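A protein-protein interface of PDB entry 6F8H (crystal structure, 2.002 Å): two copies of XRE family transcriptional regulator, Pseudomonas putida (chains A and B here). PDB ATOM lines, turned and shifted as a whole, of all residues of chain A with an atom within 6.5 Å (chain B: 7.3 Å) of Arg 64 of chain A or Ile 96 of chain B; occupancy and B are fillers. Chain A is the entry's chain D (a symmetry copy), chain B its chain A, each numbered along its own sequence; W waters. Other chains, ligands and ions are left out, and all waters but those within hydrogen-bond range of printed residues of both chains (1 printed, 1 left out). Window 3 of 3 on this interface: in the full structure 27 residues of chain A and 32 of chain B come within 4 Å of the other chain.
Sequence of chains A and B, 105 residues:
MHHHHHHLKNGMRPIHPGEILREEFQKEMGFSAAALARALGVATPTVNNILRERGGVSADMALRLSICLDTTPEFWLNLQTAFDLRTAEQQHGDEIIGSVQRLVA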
ATOM      1  N   ALA A  39      16.871 -10.167 -31.612  1.00  0.00           N
ATOM      2  CA  ALA A  39      16.542  -9.656 -30.279  1.00  0.00           C
ATOM      3  C   ALA A  39      15.425  -8.613 -30.327  1.00  0.00           C
ATOM      4  O   ALA A  39      14.598  -8.558 -29.419  1.00  0.00           O
ATOM      5  CB  ALA A  39      17.783  -9.061 -29.597  1.00  0.00           C
ATOM      6  N   LEU A  40      15.401  -7.792 -31.374  1.00  0.00           N
ATOM      7  CA  LEU A  40      14.378  -6.757 -31.504  1.00  0.00           C
ATOM      8  C   LEU A  40      13.023  -7.298 -31.956  1.00  0.00           C
ATOM      9  O   LEU A  40      11.998  -6.626 -31.808  1.00  0.00           O
ATOM     10  CB  LEU A  40      14.818  -5.681 -32.497  1.00  0.00           C
ATOM     11  CG  LEU A  40      16.005  -4.807 -32.102  1.00  0.00           C
ATOM     12  CD1 LEU A  40      16.336  -3.838 -33.233  1.00  0.00           C
ATOM     13  CD2 LEU A  40      15.689  -4.071 -30.802  1.00  0.00           C
ATOM     14  N   GLY A  41      13.020  -8.495 -32.526  1.00  0.00           N
ATOM     15  CA  GLY A  41      11.790  -9.080 -33.033  1.00  0.00           C
ATOM     16  C   GLY A  41      11.390  -8.475 -34.368  1.00  0.00           C
ATOM     17  O   GLY A  41      10.208  -8.319 -34.658  1.00  0.00           O
ATOM     18  N   VAL A  42      12.384  -8.133 -35.185  1.00  0.00           N
ATOM     19  CA  VAL A  42      12.132  -7.509 -36.467  1.00  0.00           C
ATOM     20  C   VAL A  42      13.031  -8.163 -37.496  1.00  0.00           C
ATOM     21  O   VAL A  42      13.891  -8.980 -37.150  1.00  0.00           O
ATOM     22  CB  VAL A  42      12.388  -5.966 -36.452  1.00  0.00           C
ATOM     23  CG1 VAL A  42      11.619  -5.299 -35.325  1.00  0.00           C
ATOM     24  CG2 VAL A  42      13.889  -5.662 -36.337  1.00  0.00           C
ATOM     25  N   ALA A  59       8.809   5.352 -33.755  1.00  0.00           N
ATOM     26  CA  ALA A  59       8.395   5.187 -32.368  1.00  0.00           C
ATOM     27  C   ALA A  59       8.446   3.729 -31.956  1.00  0.00           C
ATOM     28  O   ALA A  59       8.957   3.401 -30.897  1.00  0.00           O
ATOM     29  CB  ALA A  59       6.990   5.744 -32.162  1.00  0.00           C
ATOM     30  N   ASP A  60       7.915   2.850 -32.800  1.00  0.00           N
ATOM     31  CA  ASP A  60       7.930   1.424 -32.515  1.00  0.00           C
ATOM     32  C   ASP A  60       9.364   0.884 -32.373  1.00  0.00           C
ATOM     33  O   ASP A  60       9.698   0.171 -31.418  1.00  0.00           O
ATOM     34  CB  ASP A  60       7.187   0.682 -33.622  1.00  0.00           C
ATOM     35  CG  ASP A  60       6.867  -0.751 -33.257  1.00  0.00           C
ATOM     36  OD1 ASP A  60       5.773  -0.968 -32.681  1.00  0.00           O
ATOM     37  OD2 ASP A  60       7.691  -1.652 -33.567  1.00  0.00           O
ATOM     38  N   MET A  61      10.209   1.212 -33.334  1.00  0.00           N
ATOM     39  CA  MET A  61      11.600   0.802 -33.277  1.00  0.00           C
ATOM     40  C   MET A  61      12.310   1.405 -32.049  1.00  0.00           C
ATOM     41  O   MET A  61      13.116   0.747 -31.409  1.00  0.00           O
ATOM     42  CB  MET A  61      12.322   1.204 -34.556  1.00  0.00           C
ATOM     43  CG  MET A  61      13.777   0.788 -34.591  1.00  0.00           C
ATOM     44  SD  MET A  61      14.021  -0.999 -34.460  1.00  0.00           S
ATOM     45  CE  MET A  61      12.932  -1.590 -35.761  1.00  0.00           C
ATOM     46  N   ALA A  62      11.980   2.646 -31.719  1.00  0.00           N
ATOM     47  CA  ALA A  62      12.594   3.310 -30.575  1.00  0.00           C
ATOM     48  C   ALA A  62      12.269   2.561 -29.283  1.00  0.00           C
ATOM     49  O   ALA A  62      13.135   2.353 -28.449  1.00  0.00           O
ATOM     50  CB  ALA A  62      12.129   4.737 -30.485  1.00  0.00           C
ATOM     51  N   LEU A  63      11.008   2.155 -29.144  1.00  0.00           N
ATOM     52  CA  LEU A  63      10.574   1.330 -28.012  1.00  0.00           C
ATOM     53  C   LEU A  63      11.319   0.006 -27.950  1.00  0.00           C
ATOM     54  O   LEU A  63      11.814  -0.393 -26.897  1.00  0.00           O
ATOM     55  CB  LEU A  63       9.074   1.063 -28.101  1.00  0.00           C
ATOM     56  CG  LEU A  63       8.198   2.146 -27.500  1.00  0.00           C
ATOM     57  CD1 LEU A  63       6.709   1.827 -27.718  1.00  0.00           C
ATOM     58  CD2 LEU A  63       8.538   2.249 -26.011  1.00  0.00           C
ATOM     59  N   ARG A  64      11.391  -0.681 -29.082  1.00  0.00           N
ATOM     60  CA  ARG A  64      12.132  -1.933 -29.152  1.00  0.00           C
ATOM     61  C   ARG A  64      13.596  -1.722 -28.775  1.00  0.00           C
ATOM     62  O   ARG A  64      14.149  -2.478 -27.972  1.00  0.00           O
ATOM     63  CB  ARG A  64      12.019  -2.545 -30.555  1.00  0.00           C
ATOM     64  CG  ARG A  64      10.590  -2.931 -30.916  1.00  0.00           C
ATOM     65  CD  ARG A  64      10.488  -3.597 -32.286  1.00  0.00           C
ATOM     66  NE  ARG A  64       9.098  -3.958 -32.582  1.00  0.00           N
ATOM     67  CZ  ARG A  64       8.552  -5.143 -32.313  1.00  0.00           C
ATOM     68  NH1 ARG A  64       9.273  -6.095 -31.730  1.00  0.00           N
ATOM     69  NH2 ARG A  64       7.274  -5.374 -32.622  1.00  0.00           N
ATOM     70  N   LEU A  65      14.234  -0.702 -29.353  1.00  0.00           N
ATOM     71  CA  LEU A  65      15.640  -0.454 -29.034  1.00  0.00           C
ATOM     72  C   LEU A  65      15.832  -0.154 -27.552  1.00  0.00           C
ATOM     73  O   LEU A  65      16.812  -0.584 -26.954  1.00  0.00           O
ATOM     74  CB  LEU A  65      16.205   0.699 -29.864  1.00  0.00           C
ATOM     75  CG  LEU A  65      16.458   0.285 -31.312  1.00  0.00           C
ATOM     76  CD1 LEU A  65      16.414   1.508 -32.198  1.00  0.00           C
ATOM     77  CD2 LEU A  65      17.792  -0.430 -31.427  1.00  0.00           C
ATOM     78  N   SER A  66      14.880   0.559 -26.962  1.00  0.00           N
ATOM     79  CA  SER A  66      15.044   1.001 -25.591  1.00  0.00           C
ATOM     80  C   SER A  66      15.066  -0.225 -24.664  1.00  0.00           C
ATOM     81  O   SER A  66      15.933  -0.322 -23.794  1.00  0.00           O
ATOM     82  CB  SER A  66      13.942   1.987 -25.208  1.00  0.00           C
ATOM     83  OG  SER A  66      12.679   1.354 -25.175  1.00  0.00           O
ATOM     84  N   ILE A  67      14.152  -1.172 -24.888  1.00  0.00           N
ATOM     85  CA  ILE A  67      14.152  -2.430 -24.124  1.00  0.00           C
ATOM     86  C   ILE A  67      15.440  -3.220 -24.381  1.00  0.00           C
ATOM     87  O   ILE A  67      16.117  -3.671 -23.460  1.00  0.00           O
ATOM     88  CB  ILE A  67      12.925  -3.311 -24.478  1.00  0.00           C
ATOM     89  CG1 ILE A  67      11.638  -2.655 -23.978  1.00  0.00           C
ATOM     90  CG2 ILE A  67      13.048  -4.703 -23.843  1.00  0.00           C
ATOM     91  CD1 ILE A  67      10.377  -3.278 -24.518  1.00  0.00           C
ATOM     92  N   CYS A  68      15.779  -3.364 -25.652  1.00  0.00           N
ATOM     93  CA  CYS A  68      16.895  -4.194 -26.067  1.00  0.00           C
ATOM     94  C   CYS A  68      18.252  -3.698 -25.569  1.00  0.00           C
ATOM     95  O   CYS A  68      19.118  -4.503 -25.190  1.00  0.00           O
ATOM     96  CB  CYS A  68      16.909  -4.293 -27.588  1.00  0.00           C
ATOM     97  SG  CYS A  68      18.178  -5.360 -28.278  1.00  0.00           S
ATOM     98  N   LEU A  69      18.448  -2.385 -25.564  1.00  0.00           N
ATOM     99  CA  LEU A  69      19.775  -1.853 -25.276  1.00  0.00           C
ATOM    100  C   LEU A  69      19.849  -1.099 -23.939  1.00  0.00           C
ATOM    101  O   LEU A  69      20.869  -0.488 -23.629  1.00  0.00           O
ATOM    102  CB  LEU A  69      20.226  -0.952 -26.434  1.00  0.00           C
ATOM    103  CG  LEU A  69      20.298  -1.641 -27.803  1.00  0.00           C
ATOM    104  CD1 LEU A  69      20.607  -0.667 -28.939  1.00  0.00           C
ATOM    105  CD2 LEU A  69      21.297  -2.811 -27.803  1.00  0.00           C
ATOM    106  N   ALA B  88       2.355   4.454 -29.750  1.00  0.00           N
ATOM    107  CA  ALA B  88       2.978   3.151 -29.966  1.00  0.00           C
ATOM    108  C   ALA B  88       2.900   2.277 -28.706  1.00  0.00           C
ATOM    109  O   ALA B  88       2.722   1.060 -28.787  1.00  0.00           O
ATOM    110  CB  ALA B  88       4.440   3.326 -30.411  1.00  0.00           C
ATOM    111  N   GLU B  89       3.037   2.909 -27.546  1.00  0.00           N
ATOM    112  CA  GLU B  89       2.933   2.203 -26.283  1.00  0.00           C
ATOM    113  C   GLU B  89       1.507   1.721 -26.090  1.00  0.00           C
ATOM    114  O   GLU B  89       1.270   0.549 -25.761  1.00  0.00           O
ATOM    115  CB  GLU B  89       3.330   3.095 -25.114  1.00  0.00           C
ATOM    116  CG  GLU B  89       4.797   3.456 -25.009  1.00  0.00           C
ATOM    117  CD  GLU B  89       5.064   4.334 -23.791  1.00  0.00           C
ATOM    118  OE1 GLU B  89       4.445   5.415 -23.686  1.00  0.00           O
ATOM    119  OE2 GLU B  89       5.879   3.944 -22.931  1.00  0.00           O
ATOM    120  N   GLN B  91      -0.875   1.282 -28.273  1.00  0.00           N
ATOM    121  CA  GLN B  91      -1.299   0.340 -29.292  1.00  0.00           C
ATOM    122  C   GLN B  91      -0.518  -0.973 -29.237  1.00  0.00           C
ATOM    123  O   GLN B  91      -1.117  -2.048 -29.259  1.00  0.00           O
ATOM    124  CB  GLN B  91      -1.177   0.981 -30.683  1.00  0.00           C
ATOM    125  CG  GLN B  91      -2.166   2.129 -30.894  1.00  0.00           C
ATOM    126  CD  GLN B  91      -2.133   2.713 -32.304  1.00  0.00           C
ATOM    127  OE1 GLN B  91      -1.259   2.384 -33.117  1.00  0.00           O
ATOM    128  NE2 GLN B  91      -3.085   3.604 -32.595  1.00  0.00           N
ATOM    129  N   HIS B  92       0.804  -0.888 -29.135  1.00  0.00           N
ATOM    130  CA  HIS B  92       1.667  -2.060 -29.298  1.00  0.00           C
ATOM    131  C   HIS B  92       2.556  -2.380 -28.094  1.00  0.00           C
ATOM    132  O   HIS B  92       3.356  -3.313 -28.144  1.00  0.00           O
ATOM    133  CB  HIS B  92       2.563  -1.874 -30.519  1.00  0.00           C
ATOM    134  CG  HIS B  92       1.815  -1.722 -31.804  1.00  0.00           C
ATOM    135  ND1 HIS B  92       1.123  -2.762 -32.392  1.00  0.00           N
ATOM    136  CD2 HIS B  92       1.661  -0.656 -32.626  1.00  0.00           C
ATOM    137  CE1 HIS B  92       0.571  -2.340 -33.515  1.00  0.00           C
ATOM    138  NE2 HIS B  92       0.883  -1.067 -33.682  1.00  0.00           N
ATOM    139  N   GLY B  93       2.423  -1.605 -27.027  1.00  0.00           N
ATOM    140  CA  GLY B  93       3.305  -1.716 -25.879  1.00  0.00           C
ATOM    141  C   GLY B  93       3.478  -3.103 -25.277  1.00  0.00           C
ATOM    142  O   GLY B  93       4.604  -3.530 -24.995  1.00  0.00           O
ATOM    143  N   ASP B  94       2.370  -3.804 -25.067  1.00  0.00           N
ATOM    144  CA  ASP B  94       2.446  -5.119 -24.428  1.00  0.00           C
ATOM    145  C   ASP B  94       3.090  -6.131 -25.378  1.00  0.00           C
ATOM    146  O   ASP B  94       3.955  -6.909 -24.971  1.00  0.00           O
ATOM    147  CB  ASP B  94       1.057  -5.587 -23.975  1.00  0.00           C
ATOM    148  CG  ASP B  94       0.523  -4.778 -22.791  1.00  0.00           C
ATOM    149  OD1 ASP B  94       1.232  -4.661 -21.767  1.00  0.00           O
ATOM    150  OD2 ASP B  94      -0.604  -4.250 -22.887  1.00  0.00           O
ATOM    151  N   GLU B  95       2.693  -6.090 -26.645  1.00  0.00           N
ATOM    152  CA  GLU B  95       3.283  -6.956 -27.655  1.00  0.00           C
ATOM    153  C   GLU B  95       4.807  -6.776 -27.780  1.00  0.00           C
ATOM    154  O   GLU B  95       5.545  -7.743 -28.018  1.00  0.00           O
ATOM    155  CB  GLU B  95       2.627  -6.699 -29.006  1.00  0.00           C
ATOM    156  CG  GLU B  95       3.308  -7.414 -30.152  1.00  0.00           C
ATOM    157  CD  GLU B  95       3.025  -6.757 -31.489  1.00  0.00           C
ATOM    158  OE1 GLU B  95       2.069  -5.949 -31.562  1.00  0.00           O
ATOM    159  OE2 GLU B  95       3.762  -7.044 -32.462  1.00  0.00           O
ATOM    160  N   ILE B  96       5.271  -5.540 -27.621  1.00  0.00           N
ATOM    161  CA  ILE B  96       6.690  -5.239 -27.764  1.00  0.00           C
ATOM    162  C   ILE B  96       7.461  -5.785 -26.570  1.00  0.00           C
ATOM    163  O   ILE B  96       8.511  -6.409 -26.722  1.00  0.00           O
ATOM    164  CB  ILE B  96       6.919  -3.713 -27.918  1.00  0.00           C
ATOM    165  CG1 ILE B  96       6.493  -3.259 -29.323  1.00  0.00           C
ATOM    166  CG2 ILE B  96       8.371  -3.340 -27.626  1.00  0.00           C
ATOM    167  CD1 ILE B  96       6.353  -1.763 -29.486  1.00  0.00           C
ATOM    168  N   ILE B  97       6.920  -5.554 -25.380  1.00  0.00           N
ATOM    169  CA  ILE B  97       7.524  -6.016 -24.132  1.00  0.00           C
ATOM    170  C   ILE B  97       7.645  -7.541 -24.103  1.00  0.00           C
ATOM    171  O   ILE B  97       8.623  -8.094 -23.597  1.00  0.00           O
ATOM    172  CB  ILE B  97       6.700  -5.535 -22.925  1.00  0.00           C
ATOM    173  CG1 ILE B  97       6.822  -4.017 -22.796  1.00  0.00           C
ATOM    174  CG2 ILE B  97       7.151  -6.210 -21.651  1.00  0.00           C
ATOM    175  CD1 ILE B  97       5.740  -3.395 -21.943  1.00  0.00           C
ATOM    176  N   GLY B  98       6.649  -8.204 -24.679  1.00  0.00           N
ATOM    177  CA  GLY B  98       6.616  -9.650 -24.740  1.00  0.00           C
ATOM    178  C   GLY B  98       7.471 -10.275 -25.825  1.00  0.00           C
ATOM    179  O   GLY B  98       7.741 -11.473 -25.760  1.00  0.00           O
ATOM    180  N   SER B  99       7.913  -9.497 -26.811  1.00  0.00           N
ATOM    181  CA  SER B  99       8.701 -10.086 -27.893  1.00  0.00           C
ATOM    182  C   SER B  99      10.162  -9.611 -28.001  1.00  0.00           C
ATOM    183  O   SER B  99      10.924 -10.168 -28.789  1.00  0.00           O
ATOM    184  CB  SER B  99       8.003  -9.847 -29.230  1.00  0.00           C
ATOM    185  OG  SER B  99       7.922  -8.466 -29.541  1.00  0.00           O
ATOM    186  N   VAL B 100      10.560  -8.594 -27.237  1.00  0.00           N
ATOM    187  CA  VAL B 100      11.940  -8.112 -27.335  1.00  0.00           C
ATOM    188  C   VAL B 100      12.801  -8.654 -26.202  1.00  0.00           C
ATOM    189  O   VAL B 100      12.393  -8.652 -25.045  1.00  0.00           O
ATOM    190  CB  VAL B 100      12.026  -6.553 -27.334  1.00  0.00           C
ATOM    191  CG1 VAL B 100      13.482  -6.093 -27.273  1.00  0.00           C
ATOM    192  CG2 VAL B 100      11.337  -5.967 -28.566  1.00  0.00           C
ATOM    193  N   GLN B 101      13.994  -9.120 -26.554  1.00  0.00           N
ATOM    194  CA  GLN B 101      14.988  -9.573 -25.587  1.00  0.00           C
ATOM    195  C   GLN B 101      16.093  -8.520 -25.440  1.00  0.00           C
ATOM    196  O   GLN B 101      16.515  -7.939 -26.436  1.00  0.00           O
ATOM    197  CB  GLN B 101      15.589 -10.906 -26.039  1.00  0.00           C
ATOM    198  CG  GLN B 101      14.570 -12.051 -26.166  1.00  0.00           C
ATOM    199  CD  GLN B 101      14.100 -12.577 -24.812  1.00  0.00           C
ATOM    200  OE1 GLN B 101      13.154 -12.051 -24.214  1.00  0.00           O
ATOM    201  NE2 GLN B 101      14.761 -13.624 -24.327  1.00  0.00           N
ATOM    202  N   ARG B 102      16.587  -8.269 -24.227  1.00  0.00           N
ATOM    203  CA  ARG B 102      17.695  -7.328 -24.141  1.00  0.00           C
ATOM    204  C   ARG B 102      18.959  -8.020 -24.630  1.00  0.00           C
ATOM    205  O   ARG B 102      19.101  -9.237 -24.552  1.00  0.00           O
ATOM    206  CB  ARG B 102      17.867  -6.734 -22.730  1.00  0.00           C
ATOM    207  CG  ARG B 102      17.799  -7.681 -21.572  1.00  0.00           C
ATOM    208  CD  ARG B 102      17.626  -6.908 -20.250  1.00  0.00           C
ATOM    209  NE  ARG B 102      18.780  -6.067 -19.928  1.00  0.00           N
ATOM    210  CZ  ARG B 102      19.833  -6.484 -19.228  1.00  0.00           C
ATOM    211  NH1 ARG B 102      19.883  -7.738 -18.787  1.00  0.00           N
ATOM    212  NH2 ARG B 102      20.839  -5.657 -18.976  1.00  0.00           N
HETATM  213  O   HOH W   1      13.003 -11.122 -29.738  1.00  0.00           O
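The guanidinium group (NH2) of Arg 64 of chain A lies within salt-bridge range of the side-chain carboxylate (OE2) of Glu 95 of chain B (3.9 Å). OG of Ser 99 of chain B lies within hydrogen-bond range of NH1 of Arg 64 of chain A, at 3.5 Å. The backbone NH of Gln 101 of chain B lies within hydrogen-bond range of the backbone carbonyl oxygen of Ala 39 of chain A (3.0 Å). The backbone carbonyl oxygen (O) of Gln 101 of chain B lies within hydrogen-bond range of the side-chain sulfur (SG) of Cys 68 of chain A.
The backbone NH of Gly 93 of chain B sits at hydrogen-bond distance from the backbone carbonyl oxygen of Ala 88 of chain B. A ring nitrogen (ND1) of His 92 of chain B lies within hydrogen-bond range of the side-chain carboxylate of Glu 95 of chain B, at 3.4 Å. The backbone carbonyl oxygen (O) of Glu 95 of chain B lies within hydrogen-bond range of the side-chain hydroxyl (OG) of Ser 99 of chain B, at 2.9 Å. The guanidinium group (NH1) of Arg 64 of chain A is in hydrogen-bond range of the backbone carbonyl oxygen (O) of Leu 40 of chain A. The side-chain carboxylate (OD2) of Asp 60 of chain A lies within salt-bridge range of the guanidinium group (NE) of Arg 64 of chain A. The backbone carbonyl oxygen of Leu 63 of chain A is in hydrogen-bond range of the side-chain hydroxyl of Ser 66 of chain A.
CA of Val 100 of chain B touches O of Ala 39 of chain A, at 3.4 Å. Asp 60 of chain A touches His 92 of chain B. Asp 60 of chain A touches Ile 96 of chain B. Leu 63 of chain A touches Ala 88 of chain B (CD1 to CB, 3.8 Å). Ile 96 of chain B touches Arg 64 of chain A (CG2 to CG, 3.99 Å). O of Arg 64 of chain A touches CG1 of Val 100 of chain B (3.7 Å). CG2 of Ile 96 of chain B touches CD1 of Ile 67 of chain A, 3.7 Å away. Ile 67 of chain A touches Ile 97 of chain B. CG2 of Ile 67 of chain A touches CG1 of Val 100 of chain B, 3.7 Å away. Ile 67 of chain A touches Arg 102 of chain B (O to CB, 3.6 Å).
Of the printed residues of chain B, Arg 64 of chain A touches Glu 95 (3.9 Å), Ile 96 (3.99 Å), Ser 99 (3.5 Å) and Val 100 (3.7 Å). Printed residues of chain B within 4 Å of Ala 59 of chain A: Ala 88. Printed residues of chain A within 4 Å of Ile 97 of chain B: Ile 67 (3.97 Å). Printed residues of chain A within 4 Å of Gln 101 of chain B: Ala 39 (3.0 Å) and Cys 68 (3.6 Å). Of the printed residues of chain A, Val 100 of chain B touches Ala 39, Leu 40, Arg 64, Ile 67 and Cys 68. Gly 93 of chain B touches none of the printed residues of chain A. Asp 94 of chain B touches none of the printed residues of chain A. The nearest printed residue of chain B that does not touch Arg 64 of chain A is Gln 101 of chain B (6.1 Å). The nearest printed residue of chain B that does not touch Leu 63 of chain A is Ile 96 of chain B (4.02 Å).
Of the 14 printed residues of chain B, 10 touch a printed residue of chain A. Hydrophobic or aromatic side chains of chain A that line the printed part of chain B: Ala 39, Ala 59, Leu 63 and Ile 67.
No position is printed for both chains. Of the 19 pairs that touch across the chains among the printed residues, none has its exchanged pair printed and touching as well.
Water W1 bridges O of Ser 99 of chain B (2.5 Å) and O of Ala 39 of chain A (3.0 Å).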
